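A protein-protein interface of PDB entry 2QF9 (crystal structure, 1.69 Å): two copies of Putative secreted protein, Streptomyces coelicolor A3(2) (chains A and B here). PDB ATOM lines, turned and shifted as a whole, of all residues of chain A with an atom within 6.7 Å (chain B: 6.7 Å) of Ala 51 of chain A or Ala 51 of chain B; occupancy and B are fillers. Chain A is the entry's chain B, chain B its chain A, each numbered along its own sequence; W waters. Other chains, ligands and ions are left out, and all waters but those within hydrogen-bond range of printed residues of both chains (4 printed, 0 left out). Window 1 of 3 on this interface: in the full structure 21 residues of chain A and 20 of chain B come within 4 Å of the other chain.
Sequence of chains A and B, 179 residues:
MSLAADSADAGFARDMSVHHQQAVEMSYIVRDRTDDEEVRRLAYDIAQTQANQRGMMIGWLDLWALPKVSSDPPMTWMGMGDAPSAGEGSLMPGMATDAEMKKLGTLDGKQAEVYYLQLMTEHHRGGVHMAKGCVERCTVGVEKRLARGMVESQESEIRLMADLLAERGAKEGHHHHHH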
ATOM      1  N   HIS A  20      21.496  28.601   2.337  1.00  0.00           N
ATOM      2  CA  HIS A  20      20.933  28.281   3.646  1.00  0.00           C
ATOM      3  C   HIS A  20      21.349  29.255   4.738  1.00  0.00           C
ATOM      4  O   HIS A  20      20.517  29.665   5.531  1.00  0.00           O
ATOM      5  CB  HIS A  20      21.367  26.884   4.075  1.00  0.00           C
ATOM      6  CG  HIS A  20      20.475  25.802   3.565  1.00  0.00           C
ATOM      7  ND1 HIS A  20      19.781  25.892   2.373  1.00  0.00           N
ATOM      8  CD2 HIS A  20      20.178  24.587   4.083  1.00  0.00           C
ATOM      9  CE1 HIS A  20      19.074  24.792   2.199  1.00  0.00           C
ATOM     10  NE2 HIS A  20      19.309  23.979   3.214  1.00  0.00           N
ATOM     11  N   GLN A  21      22.633  29.611   4.795  1.00  0.00           N
ATOM     12  CA  GLN A  21      23.089  30.558   5.840  1.00  0.00           C
ATOM     13  C   GLN A  21      22.270  31.867   5.823  1.00  0.00           C
ATOM     14  O   GLN A  21      21.915  32.427   6.873  1.00  0.00           O
ATOM     15  CB  GLN A  21      24.584  30.876   5.711  1.00  0.00           C
ATOM     16  CG  GLN A  21      25.148  31.621   6.971  1.00  0.00           C
ATOM     17  CD  GLN A  21      24.615  31.050   8.320  1.00  0.00           C
ATOM     18  OE1 GLN A  21      24.688  29.840   8.589  1.00  0.00           O
ATOM     19  NE2 GLN A  21      24.048  31.935   9.162  1.00  0.00           N
ATOM     20  N   VAL A  24      18.754  31.299   7.308  1.00  0.00           N
ATOM     21  CA  VAL A  24      18.870  31.260   8.773  1.00  0.00           C
ATOM     22  C   VAL A  24      18.950  32.694   9.323  1.00  0.00           C
ATOM     23  O   VAL A  24      18.222  33.043  10.246  1.00  0.00           O
ATOM     24  CB  VAL A  24      20.072  30.426   9.233  1.00  0.00           C
ATOM     25  CG1 VAL A  24      20.191  30.479  10.762  1.00  0.00           C
ATOM     26  CG2 VAL A  24      19.923  28.963   8.755  1.00  0.00           C
ATOM     27  N   ILE A  46      12.309  27.089   9.858  1.00  0.00           N
ATOM     28  CA  ILE A  46      13.209  27.289   8.730  1.00  0.00           C
ATOM     29  C   ILE A  46      14.679  27.406   9.204  1.00  0.00           C
ATOM     30  O   ILE A  46      15.578  26.787   8.612  1.00  0.00           O
ATOM     31  CB  ILE A  46      12.793  28.505   7.870  1.00  0.00           C
ATOM     32  CG1 ILE A  46      11.483  28.189   7.121  1.00  0.00           C
ATOM     33  CG2 ILE A  46      13.913  28.854   6.889  1.00  0.00           C
ATOM     34  CD1 ILE A  46      10.850  29.381   6.423  1.00  0.00           C
ATOM     35  N   ALA A  47      14.924  28.204  10.249  1.00  0.00           N
ATOM     36  CA  ALA A  47      16.280  28.368  10.790  1.00  0.00           C
ATOM     37  C   ALA A  47      16.818  26.998  11.222  1.00  0.00           C
ATOM     38  O   ALA A  47      17.945  26.618  10.890  1.00  0.00           O
ATOM     39  CB  ALA A  47      16.274  29.339  11.969  1.00  0.00           C
ATOM     40  N   GLN A  48      15.988  26.238  11.921  1.00  0.00           N
ATOM     41  CA  GLN A  48      16.419  24.927  12.427  1.00  0.00           C
ATOM     42  C   GLN A  48      16.742  23.954  11.300  1.00  0.00           C
ATOM     43  O   GLN A  48      17.821  23.331  11.294  1.00  0.00           O
ATOM     44  CB  GLN A  48      15.371  24.352  13.378  1.00  0.00           C
ATOM     45  CG  GLN A  48      15.390  25.007  14.763  1.00  0.00           C
ATOM     46  CD  GLN A  48      16.604  24.595  15.597  1.00  0.00           C
ATOM     47  OE1 GLN A  48      16.518  23.663  16.409  1.00  0.00           O
ATOM     48  NE2 GLN A  48      17.728  25.252  15.386  1.00  0.00           N
ATOM     49  N   THR A  49      15.833  23.858  10.331  1.00  0.00           N
ATOM     50  CA  THR A  49      16.013  22.942   9.199  1.00  0.00           C
ATOM     51  C   THR A  49      17.232  23.331   8.370  1.00  0.00           C
ATOM     52  O   THR A  49      18.110  22.494   8.085  1.00  0.00           O
ATOM     53  CB  THR A  49      14.777  22.920   8.295  1.00  0.00           C
ATOM     54  OG1 THR A  49      13.702  22.321   9.015  1.00  0.00           O
ATOM     55  CG2 THR A  49      15.055  22.101   7.030  1.00  0.00           C
ATOM     56  N   GLN A  50      17.284  24.607   7.975  1.00  0.00           N
ATOM     57  CA  GLN A  50      18.377  25.025   7.104  1.00  0.00           C
ATOM     58  C   GLN A  50      19.754  25.028   7.813  1.00  0.00           C
ATOM     59  O   GLN A  50      20.749  24.670   7.185  1.00  0.00           O
ATOM     60  CB  GLN A  50      18.030  26.322   6.361  1.00  0.00           C
ATOM     61  CG  GLN A  50      16.746  26.134   5.512  1.00  0.00           C
ATOM     62  CD  GLN A  50      16.608  27.075   4.317  1.00  0.00           C
ATOM     63  OE1 GLN A  50      15.514  27.219   3.767  1.00  0.00           O
ATOM     64  NE2 GLN A  50      17.691  27.718   3.926  1.00  0.00           N
ATOM     65  N   ALA A  51      19.816  25.384   9.110  1.00  0.00           N
ATOM     66  CA  ALA A  51      21.082  25.287   9.866  1.00  0.00           C
ATOM     67  C   ALA A  51      21.552  23.828   9.889  1.00  0.00           C
ATOM     68  O   ALA A  51      22.730  23.543   9.687  1.00  0.00           O
ATOM     69  CB  ALA A  51      20.895  25.784  11.289  1.00  0.00           C
ATOM     70  N   ASN A  52      20.610  22.912  10.119  1.00  0.00           N
ATOM     71  CA  ASN A  52      20.933  21.498  10.184  1.00  0.00           C
ATOM     72  C   ASN A  52      21.433  20.972   8.841  1.00  0.00           C
ATOM     73  O   ASN A  52      22.467  20.299   8.786  1.00  0.00           O
ATOM     74  CB  ASN A  52      19.737  20.698  10.677  1.00  0.00           C
ATOM     75  CG  ASN A  52      20.058  19.237  10.846  1.00  0.00           C
ATOM     76  OD1 ASN A  52      20.878  18.851  11.691  1.00  0.00           O
ATOM     77  ND2 ASN A  52      19.423  18.415  10.039  1.00  0.00           N
ATOM     78  N   GLN A  53      20.737  21.340   7.763  1.00  0.00           N
ATOM     79  CA  GLN A  53      21.092  20.869   6.418  1.00  0.00           C
ATOM     80  C   GLN A  53      22.428  21.447   5.966  1.00  0.00           C
ATOM     81  O   GLN A  53      23.253  20.754   5.379  1.00  0.00           O
ATOM     82  CB  GLN A  53      19.968  21.169   5.421  1.00  0.00           C
ATOM     83  CG  GLN A  53      18.752  20.293   5.679  1.00  0.00           C
ATOM     84  CD  GLN A  53      17.572  20.580   4.770  1.00  0.00           C
ATOM     85  OE1 GLN A  53      16.641  19.757   4.666  1.00  0.00           O
ATOM     86  NE2 GLN A  53      17.587  21.718   4.106  1.00  0.00           N
ATOM     87  N   ARG A  54      22.641  22.719   6.267  1.00  0.00           N
ATOM     88  CA  ARG A  54      23.926  23.362   6.026  1.00  0.00           C
ATOM     89  C   ARG A  54      25.066  22.618   6.740  1.00  0.00           C
ATOM     90  O   ARG A  54      26.114  22.382   6.137  1.00  0.00           O
ATOM     91  CB  ARG A  54      23.868  24.814   6.473  1.00  0.00           C
ATOM     92  CG  ARG A  54      25.209  25.548   6.284  1.00  0.00           C
ATOM     93  CD  ARG A  54      25.027  27.043   6.470  1.00  0.00           C
ATOM     94  NE  ARG A  54      26.320  27.732   6.383  1.00  0.00           N
ATOM     95  CZ  ARG A  54      27.143  27.881   7.418  1.00  0.00           C
ATOM     96  NH1 ARG A  54      26.811  27.403   8.614  1.00  0.00           N
ATOM     97  NH2 ARG A  54      28.292  28.540   7.280  1.00  0.00           N
ATOM     98  N   GLY A  55      24.864  22.250   8.006  1.00  0.00           N
ATOM     99  CA  GLY A  55      25.884  21.474   8.729  1.00  0.00           C
ATOM    100  C   GLY A  55      26.175  20.140   8.041  1.00  0.00           C
ATOM    101  O   GLY A  55      27.341  19.729   7.932  1.00  0.00           O
ATOM    102  N   MET A  56      25.114  19.465   7.586  1.00  0.00           N
ATOM    103  CA  MET A  56      25.284  18.189   6.874  1.00  0.00           C
ATOM    104  C   MET A  56      26.219  18.386   5.681  1.00  0.00           C
ATOM    105  O   MET A  56      27.196  17.663   5.531  1.00  0.00           O
ATOM    106  CB  MET A  56      23.950  17.636   6.396  1.00  0.00           C
ATOM    107  CG  MET A  56      23.008  17.268   7.527  1.00  0.00           C
ATOM    108  SD  MET A  56      21.276  16.717   6.809  1.00  0.00           S
ATOM    109  CE  MET A  56      20.434  16.111   8.402  1.00  0.00           C
ATOM    110  N   HIS B  20      24.039  18.899  21.753  1.00  0.00           N
ATOM    111  CA  HIS B  20      24.025  20.151  20.989  1.00  0.00           C
ATOM    112  C   HIS B  20      22.593  20.685  20.827  1.00  0.00           C
ATOM    113  O   HIS B  20      22.333  21.889  21.013  1.00  0.00           O
ATOM    114  CB  HIS B  20      24.660  19.929  19.612  1.00  0.00           C
ATOM    115  CG  HIS B  20      26.150  20.100  19.595  1.00  0.00           C
ATOM    116  ND1 HIS B  20      26.952  19.872  20.701  1.00  0.00           N
ATOM    117  CD2 HIS B  20      26.982  20.478  18.598  1.00  0.00           C
ATOM    118  CE1 HIS B  20      28.208  20.136  20.385  1.00  0.00           C
ATOM    119  NE2 HIS B  20      28.256  20.489  19.113  1.00  0.00           N
ATOM    120  N   GLN B  21      21.668  19.790  20.487  1.00  0.00           N
ATOM    121  CA  GLN B  21      20.263  20.159  20.333  1.00  0.00           C
ATOM    122  C   GLN B  21      19.736  20.937  21.553  1.00  0.00           C
ATOM    123  O   GLN B  21      19.022  21.942  21.404  1.00  0.00           O
ATOM    124  CB  GLN B  21      19.415  18.903  20.125  1.00  0.00           C
ATOM    125  CG  GLN B  21      17.950  19.193  19.892  1.00  0.00           C
ATOM    126  CD  GLN B  21      17.169  17.922  19.609  1.00  0.00           C
ATOM    127  OE1 GLN B  21      17.079  17.020  20.456  1.00  0.00           O
ATOM    128  NE2 GLN B  21      16.595  17.841  18.403  1.00  0.00           N
ATOM    129  N   VAL B  24      21.222  24.542  21.703  1.00  0.00           N
ATOM    130  CA  VAL B  24      20.492  25.366  20.745  1.00  0.00           C
ATOM    131  C   VAL B  24      19.139  25.823  21.339  1.00  0.00           C
ATOM    132  O   VAL B  24      18.809  27.014  21.305  1.00  0.00           O
ATOM    133  CB  VAL B  24      20.318  24.620  19.382  1.00  0.00           C
ATOM    134  CG1 VAL B  24      19.454  25.460  18.423  1.00  0.00           C
ATOM    135  CG2 VAL B  24      21.714  24.301  18.784  1.00  0.00           C
ATOM    136  N   ILE B  46      26.499  30.453  20.182  1.00  0.00           N
ATOM    137  CA  ILE B  46      26.378  29.056  20.578  1.00  0.00           C
ATOM    138  C   ILE B  46      25.350  28.318  19.714  1.00  0.00           C
ATOM    139  O   ILE B  46      25.608  27.191  19.279  1.00  0.00           O
ATOM    140  CB  ILE B  46      26.035  28.933  22.082  1.00  0.00           C
ATOM    141  CG1 ILE B  46      27.245  29.390  22.901  1.00  0.00           C
ATOM    142  CG2 ILE B  46      25.617  27.474  22.445  1.00  0.00           C
ATOM    143  CD1 ILE B  46      26.981  29.473  24.413  1.00  0.00           C
ATOM    144  N   ALA B  47      24.175  28.926  19.499  1.00  0.00           N
ATOM    145  CA  ALA B  47      23.167  28.305  18.639  1.00  0.00           C
ATOM    146  C   ALA B  47      23.726  28.024  17.236  1.00  0.00           C
ATOM    147  O   ALA B  47      23.541  26.939  16.687  1.00  0.00           O
ATOM    148  CB  ALA B  47      21.908  29.186  18.541  1.00  0.00           C
ATOM    149  N   GLN B  48      24.399  29.014  16.665  1.00  0.00           N
ATOM    150  CA  GLN B  48      24.928  28.890  15.304  1.00  0.00           C
ATOM    151  C   GLN B  48      25.966  27.775  15.211  1.00  0.00           C
ATOM    152  O   GLN B  48      25.904  26.925  14.302  1.00  0.00           O
ATOM    153  CB  GLN B  48      25.478  30.232  14.813  1.00  0.00           C
ATOM    154  CG  GLN B  48      24.364  31.249  14.499  1.00  0.00           C
ATOM    155  CD  GLN B  48      23.728  30.986  13.137  1.00  0.00           C
ATOM    156  OE1 GLN B  48      24.116  31.593  12.145  1.00  0.00           O
ATOM    157  NE2 GLN B  48      22.784  30.063  13.083  1.00  0.00           N
ATOM    158  N   THR B  49      26.909  27.771  16.149  1.00  0.00           N
ATOM    159  CA  THR B  49      27.993  26.807  16.126  1.00  0.00           C
ATOM    160  C   THR B  49      27.482  25.404  16.402  1.00  0.00           C
ATOM    161  O   THR B  49      27.801  24.467  15.668  1.00  0.00           O
ATOM    162  CB  THR B  49      29.112  27.204  17.121  1.00  0.00           C
ATOM    163  OG1 THR B  49      29.670  28.443  16.680  1.00  0.00           O
ATOM    164  CG2 THR B  49      30.230  26.133  17.194  1.00  0.00           C
ATOM    165  N   GLN B  50      26.661  25.262  17.431  1.00  0.00           N
ATOM    166  CA  GLN B  50      26.210  23.936  17.845  1.00  0.00           C
ATOM    167  C   GLN B  50      25.190  23.328  16.866  1.00  0.00           C
ATOM    168  O   GLN B  50      25.257  22.137  16.575  1.00  0.00           O
ATOM    169  CB  GLN B  50      25.740  23.924  19.303  1.00  0.00           C
ATOM    170  CG  GLN B  50      26.941  24.183  20.265  1.00  0.00           C
ATOM    171  CD  GLN B  50      26.766  23.611  21.661  1.00  0.00           C
ATOM    172  OE1 GLN B  50      25.972  22.713  21.882  1.00  0.00           O
ATOM    173  NE2 GLN B  50      27.531  24.128  22.603  1.00  0.00           N
ATOM    174  N   ALA B  51      24.313  24.148  16.289  1.00  0.00           N
ATOM    175  CA  ALA B  51      23.420  23.639  15.250  1.00  0.00           C
ATOM    176  C   ALA B  51      24.237  23.173  14.055  1.00  0.00           C
ATOM    177  O   ALA B  51      23.923  22.152  13.443  1.00  0.00           O
ATOM    178  CB  ALA B  51      22.411  24.715  14.810  1.00  0.00           C
ATOM    179  N   ASN B  52      25.272  23.937  13.706  1.00  0.00           N
ATOM    180  CA  ASN B  52      26.097  23.592  12.541  1.00  0.00           C
ATOM    181  C   ASN B  52      26.826  22.270  12.795  1.00  0.00           C
ATOM    182  O   ASN B  52      26.790  21.337  11.963  1.00  0.00           O
ATOM    183  CB  ASN B  52      27.099  24.697  12.221  1.00  0.00           C
ATOM    184  CG  ASN B  52      27.896  24.400  10.970  1.00  0.00           C
ATOM    185  OD1 ASN B  52      27.325  24.228   9.882  1.00  0.00           O
ATOM    186  ND2 ASN B  52      29.205  24.323  11.110  1.00  0.00           N
ATOM    187  N   GLN B  53      27.470  22.166  13.961  1.00  0.00           N
ATOM    188  CA  GLN B  53      28.168  20.928  14.323  1.00  0.00           C
ATOM    189  C   GLN B  53      27.214  19.725  14.432  1.00  0.00           C
ATOM    190  O   GLN B  53      27.570  18.598  14.040  1.00  0.00           O
ATOM    191  CB  GLN B  53      28.947  21.115  15.617  1.00  0.00           C
ATOM    192  CG  GLN B  53      30.059  22.145  15.499  1.00  0.00           C
ATOM    193  CD  GLN B  53      30.775  22.394  16.814  1.00  0.00           C
ATOM    194  OE1 GLN B  53      30.308  21.982  17.873  1.00  0.00           O
ATOM    195  NE2 GLN B  53      31.912  23.084  16.752  1.00  0.00           N
ATOM    196  N   ARG B  54      26.011  19.962  14.966  1.00  0.00           N
ATOM    197  CA  ARG B  54      24.997  18.922  14.974  1.00  0.00           C
ATOM    198  C   ARG B  54      24.688  18.427  13.553  1.00  0.00           C
ATOM    199  O   ARG B  54      24.647  17.209  13.323  1.00  0.00           O
ATOM    200  CB  ARG B  54      23.735  19.396  15.688  1.00  0.00           C
ATOM    201  CG  ARG B  54      22.651  18.352  15.711  1.00  0.00           C
ATOM    202  CD  ARG B  54      21.500  18.776  16.602  1.00  0.00           C
ATOM    203  NE  ARG B  54      20.402  17.806  16.552  1.00  0.00           N
ATOM    204  CZ  ARG B  54      19.409  17.857  15.669  1.00  0.00           C
ATOM    205  NH1 ARG B  54      19.392  18.790  14.715  1.00  0.00           N
ATOM    206  NH2 ARG B  54      18.440  16.953  15.720  1.00  0.00           N
ATOM    207  N   GLY B  55      24.474  19.359  12.614  1.00  0.00           N
ATOM    208  CA  GLY B  55      24.277  18.992  11.204  1.00  0.00           C
ATOM    209  C   GLY B  55      25.444  18.186  10.638  1.00  0.00           C
ATOM    210  O   GLY B  55      25.225  17.215   9.913  1.00  0.00           O
ATOM    211  N   MET B  56      26.681  18.581  10.953  1.00  0.00           N
ATOM    212  CA  MET B  56      27.863  17.828  10.487  1.00  0.00           C
ATOM    213  C   MET B  56      27.795  16.369  10.950  1.00  0.00           C
ATOM    214  O   MET B  56      27.916  15.438  10.146  1.00  0.00           O
ATOM    215  CB  MET B  56      29.176  18.480  10.966  1.00  0.00           C
ATOM    216  CG  MET B  56      29.474  19.832  10.334  1.00  0.00           C
ATOM    217  SD  MET B  56      30.981  20.611  11.309  1.00  0.00           S
ATOM    218  CE  MET B  56      31.435  22.146  10.221  1.00  0.00           C
HETATM  219  O   HOH W   1      17.246  22.578  19.384  1.00  0.00           O
HETATM  220  O   HOH W   2      21.413  20.933  13.643  1.00  0.00           O
HETATM  221  O   HOH W   3      24.884  25.387   9.845  1.00  0.00           O
HETATM  222  O   HOH W   4      28.121  15.678   7.312  1.00  0.00           O
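Of the printed residues of chain B, Gln 21 of chain A touches Gln 48. Printed residues of chain B within 4 Å of Val 24 of chain A: Gln 48. Gln 50 of chain A touches none of the printed residues of chain B. Ala 51 of chain A touches just one residue of chain B: Ala 51 (3.98 Å). Printed residues of chain B within 4 Å of Asn 52 of chain A: Arg 54 (3.4 Å) and Gly 55 (3.3 Å). Of the printed residues of chain A, Val 24 of chain B touches Gln 48. Gln 50 of chain B touches none of the printed residues of chain A. Of chain A, only Ala 51 comes within 4 Å of Ala 51 of chain B. The nearest residue of chain B that does not touch Ala 51 of chain A is Asn 52 of chain B (4.4 Å).
The side-chain amide nitrogen (NE2) of Gln 21 of chain A lies within hydrogen-bond range of the side-chain amide oxygen (OE1) of Gln 48 of chain B (3.0 Å). The backbone carbonyl oxygen of Gly 55 of chain A sits close to the backbone NH of Met 56 of chain B, at 3.3 Å. NH1 of Arg 54 of chain A sits at hydrogen-bond distance from OD1 of Asn 52 of chain B (3.5 Å). NH1 of Arg 54 of chain B sits at hydrogen-bond distance from OD1 of Asn 52 of chain A (3.4 Å). The backbone NH (N) of Met 56 of chain A sits close to the backbone carbonyl oxygen (O) of Gly 55 of chain B (3.2 Å).
Of the 14 printed residues of chain A, 8 touch a printed residue of chain B. Of the 14 printed residues of chain B, 7 touch a printed residue of chain A. Printed residues of chain B that touch a printed residue of chain A: Val 24, Gln 48, Ala 51, Asn 52, Arg 54, Gly 55 and Met 56. Hydrophobic or aromatic side chains of chain B that line the printed part of chain A: Val 24, Ala 51 and Met 56. Among the printed residues, no Asp or Glu carboxylate lies within 4 Å of a Lys or Arg side-chain nitrogen of the other chain.
Gln 21 of chain A touches Gln 48 of chain B, but with the chains exchanged Gln 48 of chain A does not touch Gln 21 of chain B (5.8 Å). Ala 51 of chain A touches its own counterpart, Ala 51 of chain B. Gly 55 of chain A touches its own counterpart, Gly 55 of chain B. Gly 55 of chain A touches Met 56 of chain B, and with the chains exchanged Met 56 of chain A touches Gly 55 of chain B.
Val 24 of chain A touches Gln 48 of chain B (CG1 to NE2, 3.5 Å). Gln 48 of chain A touches Val 24 of chain B. Ala 51 of chain A touches Ala 51 of chain B. Gly 55 of chain B touches Asn 52 of chain A. CA of Gly 55 of chain A touches OD1 of Asn 52 of chain B (3.3 Å). Gly 55 of chain A touches Gly 55 of chain B (C to C, 3.3 Å). Met 56 of chain B touches Met 56 of chain A (N to N, 3.8 Å).
NE2 of Gln 21 of chain B lies close to NH2 of Arg 54 of chain B. OE1 of Gln 21 of chain A is in hydrogen-bond range of NH1 of Arg 54 of chain A (3.2 Å).
Water W3 lies within hydrogen-bond range of OD1 of Asn 52 of chain B, O of Ala 51 of chain A and NH1 of Arg 54 of chain A. Water W1 lies within hydrogen-bond range of O of Gln 21 of chain B and OE1 of Gln 48 of chain A. Water W2 lies within hydrogen-bond range of the backbone carbonyl oxygen (O) of Ala 51 of chain B, the side-chain amide oxygen (OD1) of Asn 52 of chain A and the guanidinium group (NH1) of Arg 54 of chain B. Water W4 bridges O of Met 56 of chain A (2.8 Å) and O of Met 56 of chain B (2.9 Å).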
